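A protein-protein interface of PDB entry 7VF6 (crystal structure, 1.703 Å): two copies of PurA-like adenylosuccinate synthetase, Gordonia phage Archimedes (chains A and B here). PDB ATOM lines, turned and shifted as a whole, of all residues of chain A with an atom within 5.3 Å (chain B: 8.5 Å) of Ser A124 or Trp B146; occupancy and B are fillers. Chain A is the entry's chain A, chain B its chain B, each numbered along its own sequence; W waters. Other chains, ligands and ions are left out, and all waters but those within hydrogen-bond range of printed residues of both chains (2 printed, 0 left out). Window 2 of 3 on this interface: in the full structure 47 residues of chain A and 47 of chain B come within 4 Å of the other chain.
The side-chain hydroxyl (OG) of Ser B142 is in hydrogen-bond range of the side-chain hydroxyl (OG) of Ser A142.
The indole nitrogen (NE1) of Trp B146 lies within hydrogen-bond range of the side-chain hydroxyl (OG) of Ser A142 (3.3 Å).
OG of Ser A124 sits at hydrogen-bond distance from N of Leu A126 (3.0 Å).
The backbone NH (N) of Gly A138 lies within hydrogen-bond range of the side-chain carboxylate (OE2) of Glu A121 (2.9 Å).
The backbone NH (N) of Ala A139 sits at hydrogen-bond distance from the side-chain carboxylate (OE2) of Glu A121 (2.9 Å).
The side-chain hydroxyl (OG) of Ser A124 lies within hydrogen-bond range of the backbone carbonyl oxygen (O) of Glu A121.
The backbone carbonyl oxygen (O) of Ile B145 is in hydrogen-bond range of the guanidinium group (NE) of Arg B147 (3.0 Å).
Among the printed residues, merely in contact across the chains: Ser A124 with Trp B146 (3.8 Å), Leu A126 with Trp B146 (3.5 Å), Leu A126 with Arg B147 (3.9 Å), Gly A138 with Ile B145 (3.2 Å) and Ala A139 with Trp B146 (3.7 Å).
Asp A119 touches none of the printed residues of chain B.
No residue of chain B comes within 4 Å of Ser A123.
Ser A124 touches one residue of chain B.
Of the printed residues of chain B, Leu A126 touches Trp B146 and Arg B147.
Of the printed residues of chain A, Ser B142 touches Ser A142 (2.6 Å).
Asp B143 touches none of the printed residues of chain A.
Printed residues of chain A within 4 Å of Ile B145: Gly A138 (3.2 Å).
Printed residues of chain A within 4 Å of Trp B146: Ser A124, Leu A126, Ala A139 and Ser A142.
Printed residues of chain A within 4 Å of Arg B147: Leu A126 (3.9 Å).
The nearest residue of chain B that does not touch Ser A124 is Arg B147 (8.0 Å).
The nearest printed residue of chain A that does not touch Trp B146 is Glu A121 (4.01 Å).
Of the 11 printed residues of chain B, 4 touch a printed residue of chain A.
Among the printed residues, no Asp or Glu carboxylate lies within 4 Å of a Lys or Arg side-chain nitrogen of the other chain.
Ser B142 touches its own counterpart, Ser A142.
Of the 7 pairs that touch across the chains among the printed residues, 1 has its exchanged pair printed and touching as well.
Water W1 lies within hydrogen-bond range of the side-chain carboxylate (OE2) of Glu A121 (2.6 Å), the guanidinium group (NH2) of Arg B147 (2.7 Å) and the backbone NH (N) of Gly A138 (3.3 Å).
Water W2 bridges NE1 of Trp B146 and OG of Ser A142.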
ATOM      1  N   ASP A 119      -4.444  14.016  -7.495  1.00  0.00           N
ATOM      2  CA  ASP A 119      -3.493  13.266  -6.673  1.00  0.00           C
ATOM      3  C   ASP A 119      -2.700  12.265  -7.509  1.00  0.00           C
ATOM      4  O   ASP A 119      -1.478  12.139  -7.343  1.00  0.00           O
ATOM      5  CB  ASP A 119      -4.231  12.545  -5.543  1.00  0.00           C
ATOM      6  CG  ASP A 119      -4.989  13.497  -4.620  1.00  0.00           C
ATOM      7  OD1 ASP A 119      -4.647  14.695  -4.573  1.00  0.00           O
ATOM      8  OD2 ASP A 119      -5.939  13.040  -3.936  1.00  0.00           O
ATOM      9  N   ARG A 120      -3.375  11.553  -8.423  1.00  0.00           N
ATOM     10  CA  ARG A 120      -2.692  10.550  -9.237  1.00  0.00           C
ATOM     11  C   ARG A 120      -1.596  11.171 -10.094  1.00  0.00           C
ATOM     12  O   ARG A 120      -0.531  10.575 -10.269  1.00  0.00           O
ATOM     13  CB  ARG A 120      -3.689   9.819 -10.140  1.00  0.00           C
ATOM     14  CG  ARG A 120      -4.356   8.603  -9.519  1.00  0.00           C
ATOM     15  CD  ARG A 120      -5.412   8.038 -10.462  1.00  0.00           C
ATOM     16  NE  ARG A 120      -6.393   7.230  -9.745  1.00  0.00           N
ATOM     17  CZ  ARG A 120      -7.617   6.972 -10.191  1.00  0.00           C
ATOM     18  NH1 ARG A 120      -8.017   7.461 -11.364  1.00  0.00           N
ATOM     19  NH2 ARG A 120      -8.447   6.232  -9.466  1.00  0.00           N
ATOM     20  N   GLU A 121      -1.858  12.332 -10.692  1.00  0.00           N
ATOM     21  CA  GLU A 121      -0.825  12.973 -11.496  1.00  0.00           C
ATOM     22  C   GLU A 121       0.282  13.536 -10.615  1.00  0.00           C
ATOM     23  O   GLU A 121       1.464  13.411 -10.945  1.00  0.00           O
ATOM     24  CB  GLU A 121      -1.419  14.073 -12.377  1.00  0.00           C
ATOM     25  CG  GLU A 121      -2.365  13.539 -13.448  1.00  0.00           C
ATOM     26  CD  GLU A 121      -2.529  14.498 -14.618  1.00  0.00           C
ATOM     27  OE1 GLU A 121      -2.157  15.680 -14.476  1.00  0.00           O
ATOM     28  OE2 GLU A 121      -3.018  14.067 -15.685  1.00  0.00           O
ATOM     29  N   ALA A 122      -0.086  14.168  -9.495  1.00  0.00           N
ATOM     30  CA  ALA A 122       0.915  14.836  -8.669  1.00  0.00           C
ATOM     31  C   ALA A 122       1.930  13.847  -8.114  1.00  0.00           C
ATOM     32  O   ALA A 122       3.113  14.182  -7.974  1.00  0.00           O
ATOM     33  CB  ALA A 122       0.229  15.595  -7.530  1.00  0.00           C
ATOM     34  N   SER A 123       1.505  12.627  -7.818  1.00  0.00           N
ATOM     35  CA  SER A 123       2.425  11.637  -7.275  1.00  0.00           C
ATOM     36  C   SER A 123       3.089  10.780  -8.347  1.00  0.00           C
ATOM     37  O   SER A 123       3.920   9.932  -8.008  1.00  0.00           O
ATOM     38  CB  SER A 123       1.704  10.744  -6.263  1.00  0.00           C
ATOM     39  OG  SER A 123       0.676  10.004  -6.883  1.00  0.00           O
ATOM     40  N   SER A 124       2.770  10.996  -9.620  1.00  0.00           N
ATOM     41  CA  SER A 124       3.343  10.262 -10.739  1.00  0.00           C
ATOM     42  C   SER A 124       4.635  10.916 -11.237  1.00  0.00           C
ATOM     43  O   SER A 124       5.020  12.006 -10.814  1.00  0.00           O
ATOM     44  CB  SER A 124       2.335  10.200 -11.888  1.00  0.00           C
ATOM     45  OG  SER A 124       2.424  11.383 -12.671  1.00  0.00           O
ATOM     46  N   THR A 125       5.286  10.242 -12.190  1.00  0.00           N
ATOM     47  CA  THR A 125       6.476  10.768 -12.859  1.00  0.00           C
ATOM     48  C   THR A 125       6.155  11.800 -13.944  1.00  0.00           C
ATOM     49  O   THR A 125       7.077  12.266 -14.620  1.00  0.00           O
ATOM     50  CB  THR A 125       7.294   9.613 -13.480  1.00  0.00           C
ATOM     51  OG1 THR A 125       6.521   8.954 -14.490  1.00  0.00           O
ATOM     52  CG2 THR A 125       7.722   8.580 -12.428  1.00  0.00           C
ATOM     53  N   LEU A 126       4.887  12.193 -14.115  1.00  0.00           N
ATOM     54  CA  LEU A 126       4.509  13.039 -15.251  1.00  0.00           C
ATOM     55  C   LEU A 126       5.292  14.343 -15.288  1.00  0.00           C
ATOM     56  O   LEU A 126       5.810  14.740 -16.337  1.00  0.00           O
ATOM     57  CB  LEU A 126       3.021  13.361 -15.202  1.00  0.00           C
ATOM     58  CG  LEU A 126       2.038  12.481 -15.944  1.00  0.00           C
ATOM     59  CD1 LEU A 126       0.647  13.029 -15.651  1.00  0.00           C
ATOM     60  CD2 LEU A 126       2.328  12.453 -17.449  1.00  0.00           C
ATOM     61  N   THR A 127       5.331  15.068 -14.171  1.00  0.00           N
ATOM     62  CA  THR A 127       6.031  16.348 -14.195  1.00  0.00           C
ATOM     63  C   THR A 127       7.515  16.160 -14.488  1.00  0.00           C
ATOM     64  O   THR A 127       8.092  16.884 -15.309  1.00  0.00           O
ATOM     65  CB  THR A 127       5.828  17.086 -12.877  1.00  0.00           C
ATOM     66  OG1 THR A 127       4.450  17.454 -12.763  1.00  0.00           O
ATOM     67  CG2 THR A 127       6.700  18.337 -12.836  1.00  0.00           C
ATOM     68  N   SER A 134       0.417  18.452 -13.868  1.00  0.00           N
ATOM     69  CA  SER A 134      -0.153  17.514 -12.898  1.00  0.00           C
ATOM     70  C   SER A 134      -1.429  18.058 -12.255  1.00  0.00           C
ATOM     71  O   SER A 134      -1.653  17.918 -11.051  1.00  0.00           O
ATOM     72  CB  SER A 134       0.877  17.126 -11.833  1.00  0.00           C
ATOM     73  OG  SER A 134       1.907  16.348 -12.422  1.00  0.00           O
ATOM     74  N   GLY A 138      -5.042  14.638 -17.623  1.00  0.00           N
ATOM     75  CA  GLY A 138      -4.737  13.347 -18.236  1.00  0.00           C
ATOM     76  C   GLY A 138      -5.336  12.176 -17.475  1.00  0.00           C
ATOM     77  O   GLY A 138      -5.898  11.251 -18.069  1.00  0.00           O
ATOM     78  N   ALA A 139      -5.222  12.194 -16.147  1.00  0.00           N
ATOM     79  CA  ALA A 139      -5.769  11.099 -15.356  1.00  0.00           C
ATOM     80  C   ALA A 139      -7.279  10.997 -15.533  1.00  0.00           C
ATOM     81  O   ALA A 139      -7.836   9.890 -15.589  1.00  0.00           O
ATOM     82  CB  ALA A 139      -5.405  11.287 -13.876  1.00  0.00           C
ATOM     83  N   SER A 142      -7.908   9.522 -18.972  1.00  0.00           N
ATOM     84  CA  SER A 142      -7.633   8.089 -18.942  1.00  0.00           C
ATOM     85  C   SER A 142      -8.795   7.324 -18.312  1.00  0.00           C
ATOM     86  O   SER A 142      -9.227   6.284 -18.830  1.00  0.00           O
ATOM     87  CB  SER A 142      -6.326   7.837 -18.179  1.00  0.00           C
ATOM     88  OG  SER A 142      -6.132   6.462 -17.955  1.00  0.00           O
ATOM     89  N   ALA B 139      -7.060   0.497 -23.568  1.00  0.00           N
ATOM     90  CA  ALA B 139      -5.838   0.466 -22.777  1.00  0.00           C
ATOM     91  C   ALA B 139      -4.698   1.164 -23.516  1.00  0.00           C
ATOM     92  O   ALA B 139      -3.873   1.844 -22.900  1.00  0.00           O
ATOM     93  CB  ALA B 139      -5.466  -0.980 -22.429  1.00  0.00           C
ATOM     94  N   ALA B 140      -4.648   1.025 -24.843  1.00  0.00           N
ATOM     95  CA  ALA B 140      -3.599   1.711 -25.594  1.00  0.00           C
ATOM     96  C   ALA B 140      -3.827   3.219 -25.584  1.00  0.00           C
ATOM     97  O   ALA B 140      -2.886   4.000 -25.413  1.00  0.00           O
ATOM     98  CB  ALA B 140      -3.544   1.189 -27.029  1.00  0.00           C
ATOM     99  N   ARG B 141      -5.073   3.645 -25.789  1.00  0.00           N
ATOM    100  CA  ARG B 141      -5.367   5.078 -25.748  1.00  0.00           C
ATOM    101  C   ARG B 141      -5.065   5.660 -24.376  1.00  0.00           C
ATOM    102  O   ARG B 141      -4.615   6.808 -24.265  1.00  0.00           O
ATOM    103  CB  ARG B 141      -6.834   5.312 -26.116  1.00  0.00           C
ATOM    104  CG  ARG B 141      -7.085   5.133 -27.596  1.00  0.00           C
ATOM    105  CD  ARG B 141      -8.556   5.176 -27.962  1.00  0.00           C
ATOM    106  NE  ARG B 141      -8.691   4.929 -29.392  1.00  0.00           N
ATOM    107  CZ  ARG B 141      -9.830   4.605 -29.987  1.00  0.00           C
ATOM    108  NH1 ARG B 141     -10.937   4.491 -29.268  1.00  0.00           N
ATOM    109  NH2 ARG B 141      -9.848   4.376 -31.297  1.00  0.00           N
ATOM    110  N   SER B 142      -5.332   4.892 -23.318  1.00  0.00           N
ATOM    111  CA  SER B 142      -5.033   5.353 -21.964  1.00  0.00           C
ATOM    112  C   SER B 142      -3.531   5.556 -21.770  1.00  0.00           C
ATOM    113  O   SER B 142      -3.093   6.560 -21.198  1.00  0.00           O
ATOM    114  CB  SER B 142      -5.576   4.349 -20.949  1.00  0.00           C
ATOM    115  OG  SER B 142      -5.152   4.683 -19.649  1.00  0.00           O
ATOM    116  N   ASP B 143      -2.725   4.599 -22.231  1.00  0.00           N
ATOM    117  CA  ASP B 143      -1.276   4.764 -22.169  1.00  0.00           C
ATOM    118  C   ASP B 143      -0.811   5.947 -23.017  1.00  0.00           C
ATOM    119  O   ASP B 143       0.114   6.669 -22.632  1.00  0.00           O
ATOM    120  CB  ASP B 143      -0.588   3.470 -22.608  1.00  0.00           C
ATOM    121  CG  ASP B 143      -0.397   2.482 -21.464  1.00  0.00           C
ATOM    122  OD1 ASP B 143      -0.783   2.787 -20.306  1.00  0.00           O
ATOM    123  OD2 ASP B 143       0.146   1.385 -21.735  1.00  0.00           O
ATOM    124  N   ARG B 144      -1.445   6.177 -24.174  1.00  0.00           N
ATOM    125  CA  ARG B 144      -1.080   7.345 -24.972  1.00  0.00           C
ATOM    126  C   ARG B 144      -1.365   8.634 -24.204  1.00  0.00           C
ATOM    127  O   ARG B 144      -0.569   9.582 -24.233  1.00  0.00           O
ATOM    128  CB  ARG B 144      -1.832   7.321 -26.307  1.00  0.00           C
ATOM    129  CG  ARG B 144      -1.425   8.441 -27.287  1.00  0.00           C
ATOM    130  CD  ARG B 144       0.010   8.231 -27.743  1.00  0.00           C
ATOM    131  NE  ARG B 144       0.521   9.283 -28.630  1.00  0.00           N
ATOM    132  CZ  ARG B 144       0.491   9.211 -29.962  1.00  0.00           C
ATOM    133  NH1 ARG B 144      -0.037   8.143 -30.561  1.00  0.00           N
ATOM    134  NH2 ARG B 144       1.015  10.194 -30.694  1.00  0.00           N
ATOM    135  N   ILE B 145      -2.505   8.682 -23.507  1.00  0.00           N
ATOM    136  CA  ILE B 145      -2.874   9.859 -22.717  1.00  0.00           C
ATOM    137  C   ILE B 145      -1.863  10.105 -21.599  1.00  0.00           C
ATOM    138  O   ILE B 145      -1.508  11.255 -21.308  1.00  0.00           O
ATOM    139  CB  ILE B 145      -4.299   9.685 -22.158  1.00  0.00           C
ATOM    140  CG1 ILE B 145      -5.355  10.028 -23.210  1.00  0.00           C
ATOM    141  CG2 ILE B 145      -4.515  10.525 -20.914  1.00  0.00           C
ATOM    142  CD1 ILE B 145      -6.713   9.443 -22.836  1.00  0.00           C
ATOM    143  N   TRP B 146      -1.394   9.035 -20.949  1.00  0.00           N
ATOM    144  CA  TRP B 146      -0.374   9.149 -19.910  1.00  0.00           C
ATOM    145  C   TRP B 146       1.022   9.323 -20.486  1.00  0.00           C
ATOM    146  O   TRP B 146       1.990   9.438 -19.721  1.00  0.00           O
ATOM    147  CB  TRP B 146      -0.409   7.921 -18.993  1.00  0.00           C
ATOM    148  CG  TRP B 146      -1.432   8.008 -17.899  1.00  0.00           C
ATOM    149  CD1 TRP B 146      -2.709   7.488 -17.903  1.00  0.00           C
ATOM    150  CD2 TRP B 146      -1.264   8.645 -16.633  1.00  0.00           C
ATOM    151  NE1 TRP B 146      -3.334   7.775 -16.718  1.00  0.00           N
ATOM    152  CE2 TRP B 146      -2.463   8.473 -15.917  1.00  0.00           C
ATOM    153  CE3 TRP B 146      -0.197   9.322 -16.024  1.00  0.00           C
ATOM    154  CZ2 TRP B 146      -2.643   8.986 -14.629  1.00  0.00           C
ATOM    155  CZ3 TRP B 146      -0.374   9.825 -14.745  1.00  0.00           C
ATOM    156  CH2 TRP B 146      -1.587   9.655 -14.062  1.00  0.00           C
ATOM    157  N   ARG B 147       1.139   9.345 -21.814  1.00  0.00           N
ATOM    158  CA  ARG B 147       2.409   9.508 -22.502  1.00  0.00           C
ATOM    159  C   ARG B 147       3.397   8.401 -22.132  1.00  0.00           C
ATOM    160  O   ARG B 147       4.610   8.613 -22.133  1.00  0.00           O
ATOM    161  CB  ARG B 147       2.983  10.909 -22.252  1.00  0.00           C
ATOM    162  CG  ARG B 147       2.319  11.981 -23.154  1.00  0.00           C
ATOM    163  CD  ARG B 147       1.958  13.288 -22.423  1.00  0.00           C
ATOM    164  NE  ARG B 147       0.878  13.090 -21.469  1.00  0.00           N
ATOM    165  CZ  ARG B 147       0.451  13.990 -20.585  1.00  0.00           C
ATOM    166  NH1 ARG B 147       0.998  15.204 -20.501  1.00  0.00           N
ATOM    167  NH2 ARG B 147      -0.532  13.663 -19.767  1.00  0.00           N
ATOM    168  N   VAL B 148       2.886   7.197 -21.849  1.00  0.00           N
ATOM    169  CA  VAL B 148       3.735   6.018 -21.667  1.00  0.00           C
ATOM    170  C   VAL B 148       3.637   5.023 -22.819  1.00  0.00           C
ATOM    171  O   VAL B 148       4.442   4.085 -22.867  1.00  0.00           O
ATOM    172  CB  VAL B 148       3.448   5.303 -20.329  1.00  0.00           C
ATOM    173  CG1 VAL B 148       3.626   6.262 -19.159  1.00  0.00           C
ATOM    174  CG2 VAL B 148       2.056   4.678 -20.305  1.00  0.00           C
ATOM    175  N   ALA B 149       2.698   5.190 -23.748  1.00  0.00           N
ATOM    176  CA  ALA B 149       2.629   4.289 -24.888  1.00  0.00           C
ATOM    177  C   ALA B 149       3.835   4.477 -25.799  1.00  0.00           C
ATOM    178  O   ALA B 149       4.454   5.544 -25.842  1.00  0.00           O
ATOM    179  CB  ALA B 149       1.346   4.525 -25.687  1.00  0.00           C
HETATM  180  O   HOH W   1      -1.751  14.963 -17.764  1.00  0.00           O
HETATM  181  O   HOH W   2      -4.986   6.078 -14.885  1.00  0.00           O
